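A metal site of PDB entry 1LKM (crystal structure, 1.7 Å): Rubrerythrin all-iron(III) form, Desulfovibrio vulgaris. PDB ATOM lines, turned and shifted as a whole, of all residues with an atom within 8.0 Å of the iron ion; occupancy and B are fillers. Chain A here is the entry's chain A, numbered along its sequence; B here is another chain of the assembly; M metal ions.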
ATOM      1  N   ARG A 157     -11.064   0.470  17.386  1.00  0.00           N
ATOM      2  CA  ARG A 157     -10.590  -0.496  16.403  1.00  0.00           C
ATOM      3  C   ARG A 157      -9.471  -1.349  16.976  1.00  0.00           C
ATOM      4  O   ARG A 157      -8.586  -0.848  17.661  1.00  0.00           O
ATOM      5  CB  ARG A 157     -10.073   0.218  15.152  1.00  0.00           C
ATOM      6  CG  ARG A 157      -9.736  -0.739  14.001  1.00  0.00           C
ATOM      7  CD  ARG A 157      -9.090  -0.027  12.821  1.00  0.00           C
ATOM      8  NE  ARG A 157      -7.718   0.390  13.113  1.00  0.00           N
ATOM      9  CZ  ARG A 157      -6.647  -0.003  12.433  1.00  0.00           C
ATOM     10  NH1 ARG A 157      -6.776  -0.822  11.404  1.00  0.00           N
ATOM     11  NH2 ARG A 157      -5.439   0.431  12.785  1.00  0.00           N
ATOM     12  N   CYS A 158      -9.519  -2.656  16.690  1.00  0.00           N
ATOM     13  CA  CYS A 158      -8.483  -3.563  17.135  1.00  0.00           C
ATOM     14  C   CYS A 158      -7.346  -3.433  16.119  1.00  0.00           C
ATOM     15  O   CYS A 158      -7.547  -3.656  14.932  1.00  0.00           O
ATOM     16  CB  CYS A 158      -8.998  -5.006  17.147  1.00  0.00           C
ATOM     17  SG  CYS A 158      -7.706  -6.208  17.538  1.00  0.00           S
ATOM     18  N   ARG A 159      -6.154  -3.050  16.580  1.00  0.00           N
ATOM     19  CA  ARG A 159      -5.031  -2.906  15.665  1.00  0.00           C
ATOM     20  C   ARG A 159      -4.538  -4.247  15.140  1.00  0.00           C
ATOM     21  O   ARG A 159      -3.938  -4.315  14.062  1.00  0.00           O
ATOM     22  CB  ARG A 159      -3.877  -2.165  16.351  1.00  0.00           C
ATOM     23  CG  ARG A 159      -4.136  -0.680  16.588  1.00  0.00           C
ATOM     24  CD  ARG A 159      -2.945   0.003  17.236  1.00  0.00           C
ATOM     25  NE  ARG A 159      -1.746  -0.053  16.400  1.00  0.00           N
ATOM     26  CZ  ARG A 159      -1.563   0.655  15.296  1.00  0.00           C
ATOM     27  NH1 ARG A 159      -2.488   1.502  14.872  1.00  0.00           N
ATOM     28  NH2 ARG A 159      -0.435   0.511  14.596  1.00  0.00           N
ATOM     29  N   ASN A 160      -4.820  -5.322  15.877  1.00  0.00           N
ATOM     30  CA  ASN A 160      -4.372  -6.640  15.461  1.00  0.00           C
ATOM     31  C   ASN A 160      -5.166  -7.246  14.301  1.00  0.00           C
ATOM     32  O   ASN A 160      -4.566  -7.824  13.381  1.00  0.00           O
ATOM     33  CB  ASN A 160      -4.425  -7.612  16.661  1.00  0.00           C
ATOM     34  CG  ASN A 160      -3.762  -8.950  16.359  1.00  0.00           C
ATOM     35  OD1 ASN A 160      -4.393 -10.001  16.417  1.00  0.00           O
ATOM     36  ND2 ASN A 160      -2.473  -8.901  16.035  1.00  0.00           N
ATOM     37  N   CYS A 161      -6.490  -7.100  14.313  1.00  0.00           N
ATOM     38  CA  CYS A 161      -7.321  -7.690  13.262  1.00  0.00           C
ATOM     39  C   CYS A 161      -8.293  -6.756  12.544  1.00  0.00           C
ATOM     40  O   CYS A 161      -8.895  -7.157  11.541  1.00  0.00           O
ATOM     41  CB  CYS A 161      -8.102  -8.874  13.828  1.00  0.00           C
ATOM     42  SG  CYS A 161      -9.509  -8.419  14.869  1.00  0.00           S
ATOM     43  N   GLY A 162      -8.474  -5.548  13.060  1.00  0.00           N
ATOM     44  CA  GLY A 162      -9.375  -4.606  12.416  1.00  0.00           C
ATOM     45  C   GLY A 162     -10.800  -4.599  12.943  1.00  0.00           C
ATOM     46  O   GLY A 162     -11.644  -3.858  12.438  1.00  0.00           O
ATOM     47  N   TYR A 163     -11.085  -5.420  13.947  1.00  0.00           N
ATOM     48  CA  TYR A 163     -12.436  -5.441  14.500  1.00  0.00           C
ATOM     49  C   TYR A 163     -12.814  -4.064  15.032  1.00  0.00           C
ATOM     50  O   TYR A 163     -11.983  -3.362  15.600  1.00  0.00           O
ATOM     51  CB  TYR A 163     -12.527  -6.461  15.641  1.00  0.00           C
ATOM     52  CG  TYR A 163     -13.902  -6.508  16.277  1.00  0.00           C
ATOM     53  CD1 TYR A 163     -14.968  -7.110  15.623  1.00  0.00           C
ATOM     54  CD2 TYR A 163     -14.136  -5.904  17.516  1.00  0.00           C
ATOM     55  CE1 TYR A 163     -16.254  -7.104  16.179  1.00  0.00           C
ATOM     56  CE2 TYR A 163     -15.402  -5.891  18.079  1.00  0.00           C
ATOM     57  CZ  TYR A 163     -16.456  -6.493  17.405  1.00  0.00           C
ATOM     58  OH  TYR A 163     -17.721  -6.493  17.963  1.00  0.00           O
ATOM     59  N   VAL A 164     -14.076  -3.676  14.824  1.00  0.00           N
ATOM     60  CA  VAL A 164     -14.566  -2.384  15.298  1.00  0.00           C
ATOM     61  C   VAL A 164     -15.586  -2.611  16.409  1.00  0.00           C
ATOM     62  O   VAL A 164     -16.569  -3.320  16.223  1.00  0.00           O
ATOM     63  CB  VAL A 164     -15.213  -1.573  14.160  1.00  0.00           C
ATOM     64  CG1 VAL A 164     -15.790  -0.270  14.708  1.00  0.00           C
ATOM     65  CG2 VAL A 164     -14.184  -1.280  13.077  1.00  0.00           C
ATOM     66  N   LEU A 173     -11.317  -8.197  25.699  1.00  0.00           N
ATOM     67  CA  LEU A 173     -10.807  -9.118  24.687  1.00  0.00           C
ATOM     68  C   LEU A 173     -11.489  -8.844  23.357  1.00  0.00           C
ATOM     69  O   LEU A 173     -12.684  -8.589  23.308  1.00  0.00           O
ATOM     70  CB  LEU A 173     -11.087 -10.575  25.094  1.00  0.00           C
ATOM     71  CG  LEU A 173     -10.326 -11.174  26.276  1.00  0.00           C
ATOM     72  CD1 LEU A 173     -10.843 -12.586  26.542  1.00  0.00           C
ATOM     73  CD2 LEU A 173      -8.840 -11.196  25.976  1.00  0.00           C
ATOM     74  N   CYS A 174     -10.715  -8.882  22.274  1.00  0.00           N
ATOM     75  CA  CYS A 174     -11.306  -8.658  20.955  1.00  0.00           C
ATOM     76  C   CYS A 174     -12.148  -9.883  20.634  1.00  0.00           C
ATOM     77  O   CYS A 174     -11.664 -11.011  20.676  1.00  0.00           O
ATOM     78  CB  CYS A 174     -10.210  -8.506  19.895  1.00  0.00           C
ATOM     79  SG  CYS A 174     -10.879  -8.326  18.223  1.00  0.00           S
ATOM     80  N   PRO A 175     -13.445  -9.681  20.311  1.00  0.00           N
ATOM     81  CA  PRO A 175     -14.286 -10.829  19.989  1.00  0.00           C
ATOM     82  C   PRO A 175     -13.901 -11.558  18.710  1.00  0.00           C
ATOM     83  O   PRO A 175     -14.288 -12.698  18.497  1.00  0.00           O
ATOM     84  CB  PRO A 175     -15.692 -10.216  19.919  1.00  0.00           C
ATOM     85  CG  PRO A 175     -15.431  -8.834  19.466  1.00  0.00           C
ATOM     86  CD  PRO A 175     -14.217  -8.424  20.272  1.00  0.00           C
ATOM     87  N   ALA A 176     -13.119 -10.900  17.854  1.00  0.00           N
ATOM     88  CA  ALA A 176     -12.689 -11.523  16.605  1.00  0.00           C
ATOM     89  C   ALA A 176     -11.378 -12.299  16.743  1.00  0.00           C
ATOM     90  O   ALA A 176     -11.336 -13.493  16.478  1.00  0.00           O
ATOM     91  CB  ALA A 176     -12.555 -10.462  15.502  1.00  0.00           C
ATOM     92  N   CYS A 177     -10.311 -11.629  17.184  1.00  0.00           N
ATOM     93  CA  CYS A 177      -9.003 -12.284  17.304  1.00  0.00           C
ATOM     94  C   CYS A 177      -8.570 -12.685  18.717  1.00  0.00           C
ATOM     95  O   CYS A 177      -7.469 -13.219  18.898  1.00  0.00           O
ATOM     96  CB  CYS A 177      -7.910 -11.408  16.691  1.00  0.00           C
ATOM     97  SG  CYS A 177      -7.507  -9.955  17.670  1.00  0.00           S
ATOM     98  N   ALA A 178      -9.425 -12.433  19.705  1.00  0.00           N
ATOM     99  CA  ALA A 178      -9.145 -12.791  21.092  1.00  0.00           C
ATOM    100  C   ALA A 178      -7.943 -12.107  21.720  1.00  0.00           C
ATOM    101  O   ALA A 178      -7.474 -12.515  22.785  1.00  0.00           O
ATOM    102  CB  ALA A 178      -9.007 -14.306  21.223  1.00  0.00           C
ATOM    103  N   HIS A 179      -7.421 -11.064  21.075  1.00  0.00           N
ATOM    104  CA  HIS A 179      -6.289 -10.346  21.658  1.00  0.00           C
ATOM    105  C   HIS A 179      -6.803  -9.393  22.727  1.00  0.00           C
ATOM    106  O   HIS A 179      -7.963  -8.964  22.689  1.00  0.00           O
ATOM    107  CB  HIS A 179      -5.491  -9.617  20.583  1.00  0.00           C
ATOM    108  CG  HIS A 179      -4.515 -10.489  19.864  1.00  0.00           C
ATOM    109  ND1 HIS A 179      -4.891 -11.650  19.217  1.00  0.00           N
ATOM    110  CD2 HIS A 179      -3.167 -10.407  19.741  1.00  0.00           C
ATOM    111  CE1 HIS A 179      -3.818 -12.240  18.732  1.00  0.00           C
ATOM    112  NE2 HIS A 179      -2.757 -11.507  19.032  1.00  0.00           N
ATOM    113  N   PRO A 180      -5.960  -9.067  23.717  1.00  0.00           N
ATOM    114  CA  PRO A 180      -6.341  -8.164  24.804  1.00  0.00           C
ATOM    115  C   PRO A 180      -6.617  -6.717  24.429  1.00  0.00           C
ATOM    116  O   PRO A 180      -6.213  -6.236  23.368  1.00  0.00           O
ATOM    117  CB  PRO A 180      -5.181  -8.297  25.785  1.00  0.00           C
ATOM    118  CG  PRO A 180      -4.021  -8.508  24.889  1.00  0.00           C
ATOM    119  CD  PRO A 180      -4.567  -9.513  23.885  1.00  0.00           C
ATOM    120  N   HIS A 183      -4.631  -3.849  22.424  1.00  0.00           N
ATOM    121  CA  HIS A 183      -4.548  -3.635  20.989  1.00  0.00           C
ATOM    122  C   HIS A 183      -5.520  -2.603  20.410  1.00  0.00           C
ATOM    123  O   HIS A 183      -5.405  -2.232  19.244  1.00  0.00           O
ATOM    124  CB  HIS A 183      -4.727  -4.970  20.258  1.00  0.00           C
ATOM    125  CG  HIS A 183      -3.586  -5.919  20.477  1.00  0.00           C
ATOM    126  ND1 HIS A 183      -2.528  -6.020  19.593  1.00  0.00           N
ATOM    127  CD2 HIS A 183      -3.306  -6.760  21.504  1.00  0.00           C
ATOM    128  CE1 HIS A 183      -1.645  -6.880  20.080  1.00  0.00           C
ATOM    129  NE2 HIS A 183      -2.096  -7.337  21.229  1.00  0.00           N
ATOM    130  N   PHE A 184      -6.465  -2.134  21.214  1.00  0.00           N
ATOM    131  CA  PHE A 184      -7.449  -1.175  20.724  1.00  0.00           C
ATOM    132  C   PHE A 184      -7.053   0.297  20.732  1.00  0.00           C
ATOM    133  O   PHE A 184      -6.268   0.752  21.553  1.00  0.00           O
ATOM    134  CB  PHE A 184      -8.766  -1.330  21.494  1.00  0.00           C
ATOM    135  CG  PHE A 184      -9.551  -2.555  21.108  1.00  0.00           C
ATOM    136  CD1 PHE A 184      -9.279  -3.788  21.712  1.00  0.00           C
ATOM    137  CD2 PHE A 184     -10.538  -2.485  20.127  1.00  0.00           C
ATOM    138  CE1 PHE A 184      -9.992  -4.933  21.330  1.00  0.00           C
ATOM    139  CE2 PHE A 184     -11.253  -3.617  19.750  1.00  0.00           C
ATOM    140  CZ  PHE A 184     -10.980  -4.849  20.353  1.00  0.00           C
ATOM    141  N   GLN B  52      -3.692  -8.095   9.115  1.00  0.00           N
ATOM    142  CA  GLN B  52      -4.912  -8.379   9.864  1.00  0.00           C
ATOM    143  C   GLN B  52      -5.562  -9.651   9.312  1.00  0.00           C
ATOM    144  O   GLN B  52      -6.151 -10.412  10.079  1.00  0.00           O
ATOM    145  CB  GLN B  52      -5.852  -7.159   9.829  1.00  0.00           C
ATOM    146  CG  GLN B  52      -5.150  -5.925  10.410  1.00  0.00           C
ATOM    147  CD  GLN B  52      -6.043  -4.720  10.599  1.00  0.00           C
ATOM    148  OE1 GLN B  52      -6.944  -4.463   9.799  1.00  0.00           O
ATOM    149  NE2 GLN B  52      -5.790  -3.948  11.656  1.00  0.00           N
ATOM    150  N   GLU B  55      -4.098 -12.503  10.952  1.00  0.00           N
ATOM    151  CA  GLU B  55      -4.650 -12.741  12.278  1.00  0.00           C
ATOM    152  C   GLU B  55      -6.038 -13.400  12.236  1.00  0.00           C
ATOM    153  O   GLU B  55      -6.349 -14.239  13.084  1.00  0.00           O
ATOM    154  CB  GLU B  55      -4.684 -11.429  13.064  1.00  0.00           C
ATOM    155  CG  GLU B  55      -3.275 -10.857  13.317  1.00  0.00           C
ATOM    156  CD  GLU B  55      -2.390 -11.837  14.075  1.00  0.00           C
ATOM    157  OE1 GLU B  55      -2.847 -12.357  15.109  1.00  0.00           O
ATOM    158  OE2 GLU B  55      -1.248 -12.072  13.649  1.00  0.00           O
ATOM    159  N   HIS B  56      -6.869 -13.036  11.274  1.00  0.00           N
ATOM    160  CA  HIS B  56      -8.177 -13.682  11.155  1.00  0.00           C
ATOM    161  C   HIS B  56      -7.904 -15.155  10.849  1.00  0.00           C
ATOM    162  O   HIS B  56      -8.532 -16.061  11.416  1.00  0.00           O
ATOM    163  CB  HIS B  56      -8.980 -13.075  10.001  1.00  0.00           C
ATOM    164  CG  HIS B  56      -9.488 -11.696  10.286  1.00  0.00           C
ATOM    165  ND1 HIS B  56      -9.753 -10.782   9.292  1.00  0.00           N
ATOM    166  CD2 HIS B  56      -9.772 -11.076  11.455  1.00  0.00           C
ATOM    167  CE1 HIS B  56     -10.171  -9.649   9.837  1.00  0.00           C
ATOM    168  NE2 HIS B  56     -10.192  -9.801  11.145  1.00  0.00           N
ATOM    169  N   ARG B  59      -6.764 -17.156  13.994  1.00  0.00           N
ATOM    170  CA  ARG B  59      -7.874 -17.491  14.878  1.00  0.00           C
ATOM    171  C   ARG B  59      -8.615 -18.697  14.312  1.00  0.00           C
ATOM    172  O   ARG B  59      -8.972 -19.628  15.036  1.00  0.00           O
ATOM    173  CB  ARG B  59      -8.842 -16.301  15.012  1.00  0.00           C
ATOM    174  CG  ARG B  59      -9.967 -16.526  16.036  1.00  0.00           C
ATOM    175  CD  ARG B  59      -9.408 -16.633  17.440  1.00  0.00           C
ATOM    176  NE  ARG B  59     -10.359 -17.155  18.424  1.00  0.00           N
ATOM    177  CZ  ARG B  59     -11.335 -16.455  18.997  1.00  0.00           C
ATOM    178  NH1 ARG B  59     -11.509 -15.176  18.685  1.00  0.00           N
ATOM    179  NH2 ARG B  59     -12.125 -17.024  19.897  1.00  0.00           N
ATOM    180  N   SER B 123     -17.904 -11.811  14.172  1.00  0.00           N
ATOM    181  CA  SER B 123     -17.028 -10.734  14.604  1.00  0.00           C
ATOM    182  C   SER B 123     -16.025 -10.377  13.509  1.00  0.00           C
ATOM    183  O   SER B 123     -15.753  -9.200  13.272  1.00  0.00           O
ATOM    184  CB  SER B 123     -16.300 -11.129  15.883  1.00  0.00           C
ATOM    185  OG  SER B 123     -17.218 -11.251  16.959  1.00  0.00           O
ATOM    186  N   ALA B 127     -14.886  -6.623  11.013  1.00  0.00           N
ATOM    187  CA  ALA B 127     -13.586  -6.094  10.610  1.00  0.00           C
ATOM    188  C   ALA B 127     -13.529  -5.958   9.094  1.00  0.00           C
ATOM    189  O   ALA B 127     -13.011  -4.970   8.570  1.00  0.00           O
ATOM    190  CB  ALA B 127     -12.470  -7.010  11.090  1.00  0.00           C
HETATM  191 FE    FE M   1      -8.867  -8.197  17.028  1.00  0.00          FE
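N of Tyr 163 sits close to SG of Cys 161 (3.5 Å).
A ring nitrogen (NE2) of His 56 of chain B lies within hydrogen-bond range of the backbone carbonyl oxygen of Cys 161 (3.0 Å).
SG of Cys 177 lies close to OD1 of Asn 160 (3.4 Å).
O of Cys 177 is in hydrogen-bond range of ND1 of His 179 (3.0 Å).
The backbone NH (N) of Ala 176 sits close to the side-chain sulfur (SG) of Cys 174, 3.4 Å away.
The backbone NH of Cys 174 is in hydrogen-bond range of the backbone carbonyl oxygen of His 179.
N of Cys 158 lies within hydrogen-bond range of O of Tyr 163 (2.8 Å).
SG of Cys 158 sits close to N of Asn 160.
The iron ion is bound by the side-chain sulfur of Cys 161 (2.3 Å), the side-chain sulfur of Cys 177 (2.3 Å), the side-chain sulfur of Cys 174 (2.3 Å) and the side-chain sulfur of Cys 158 (2.4 Å).
The iron ion has four donor atoms within binding distance.
Four residues have an atom within 4 Å of the iron ion: Cys 158, Cys 161, Cys 174 and Cys 177.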
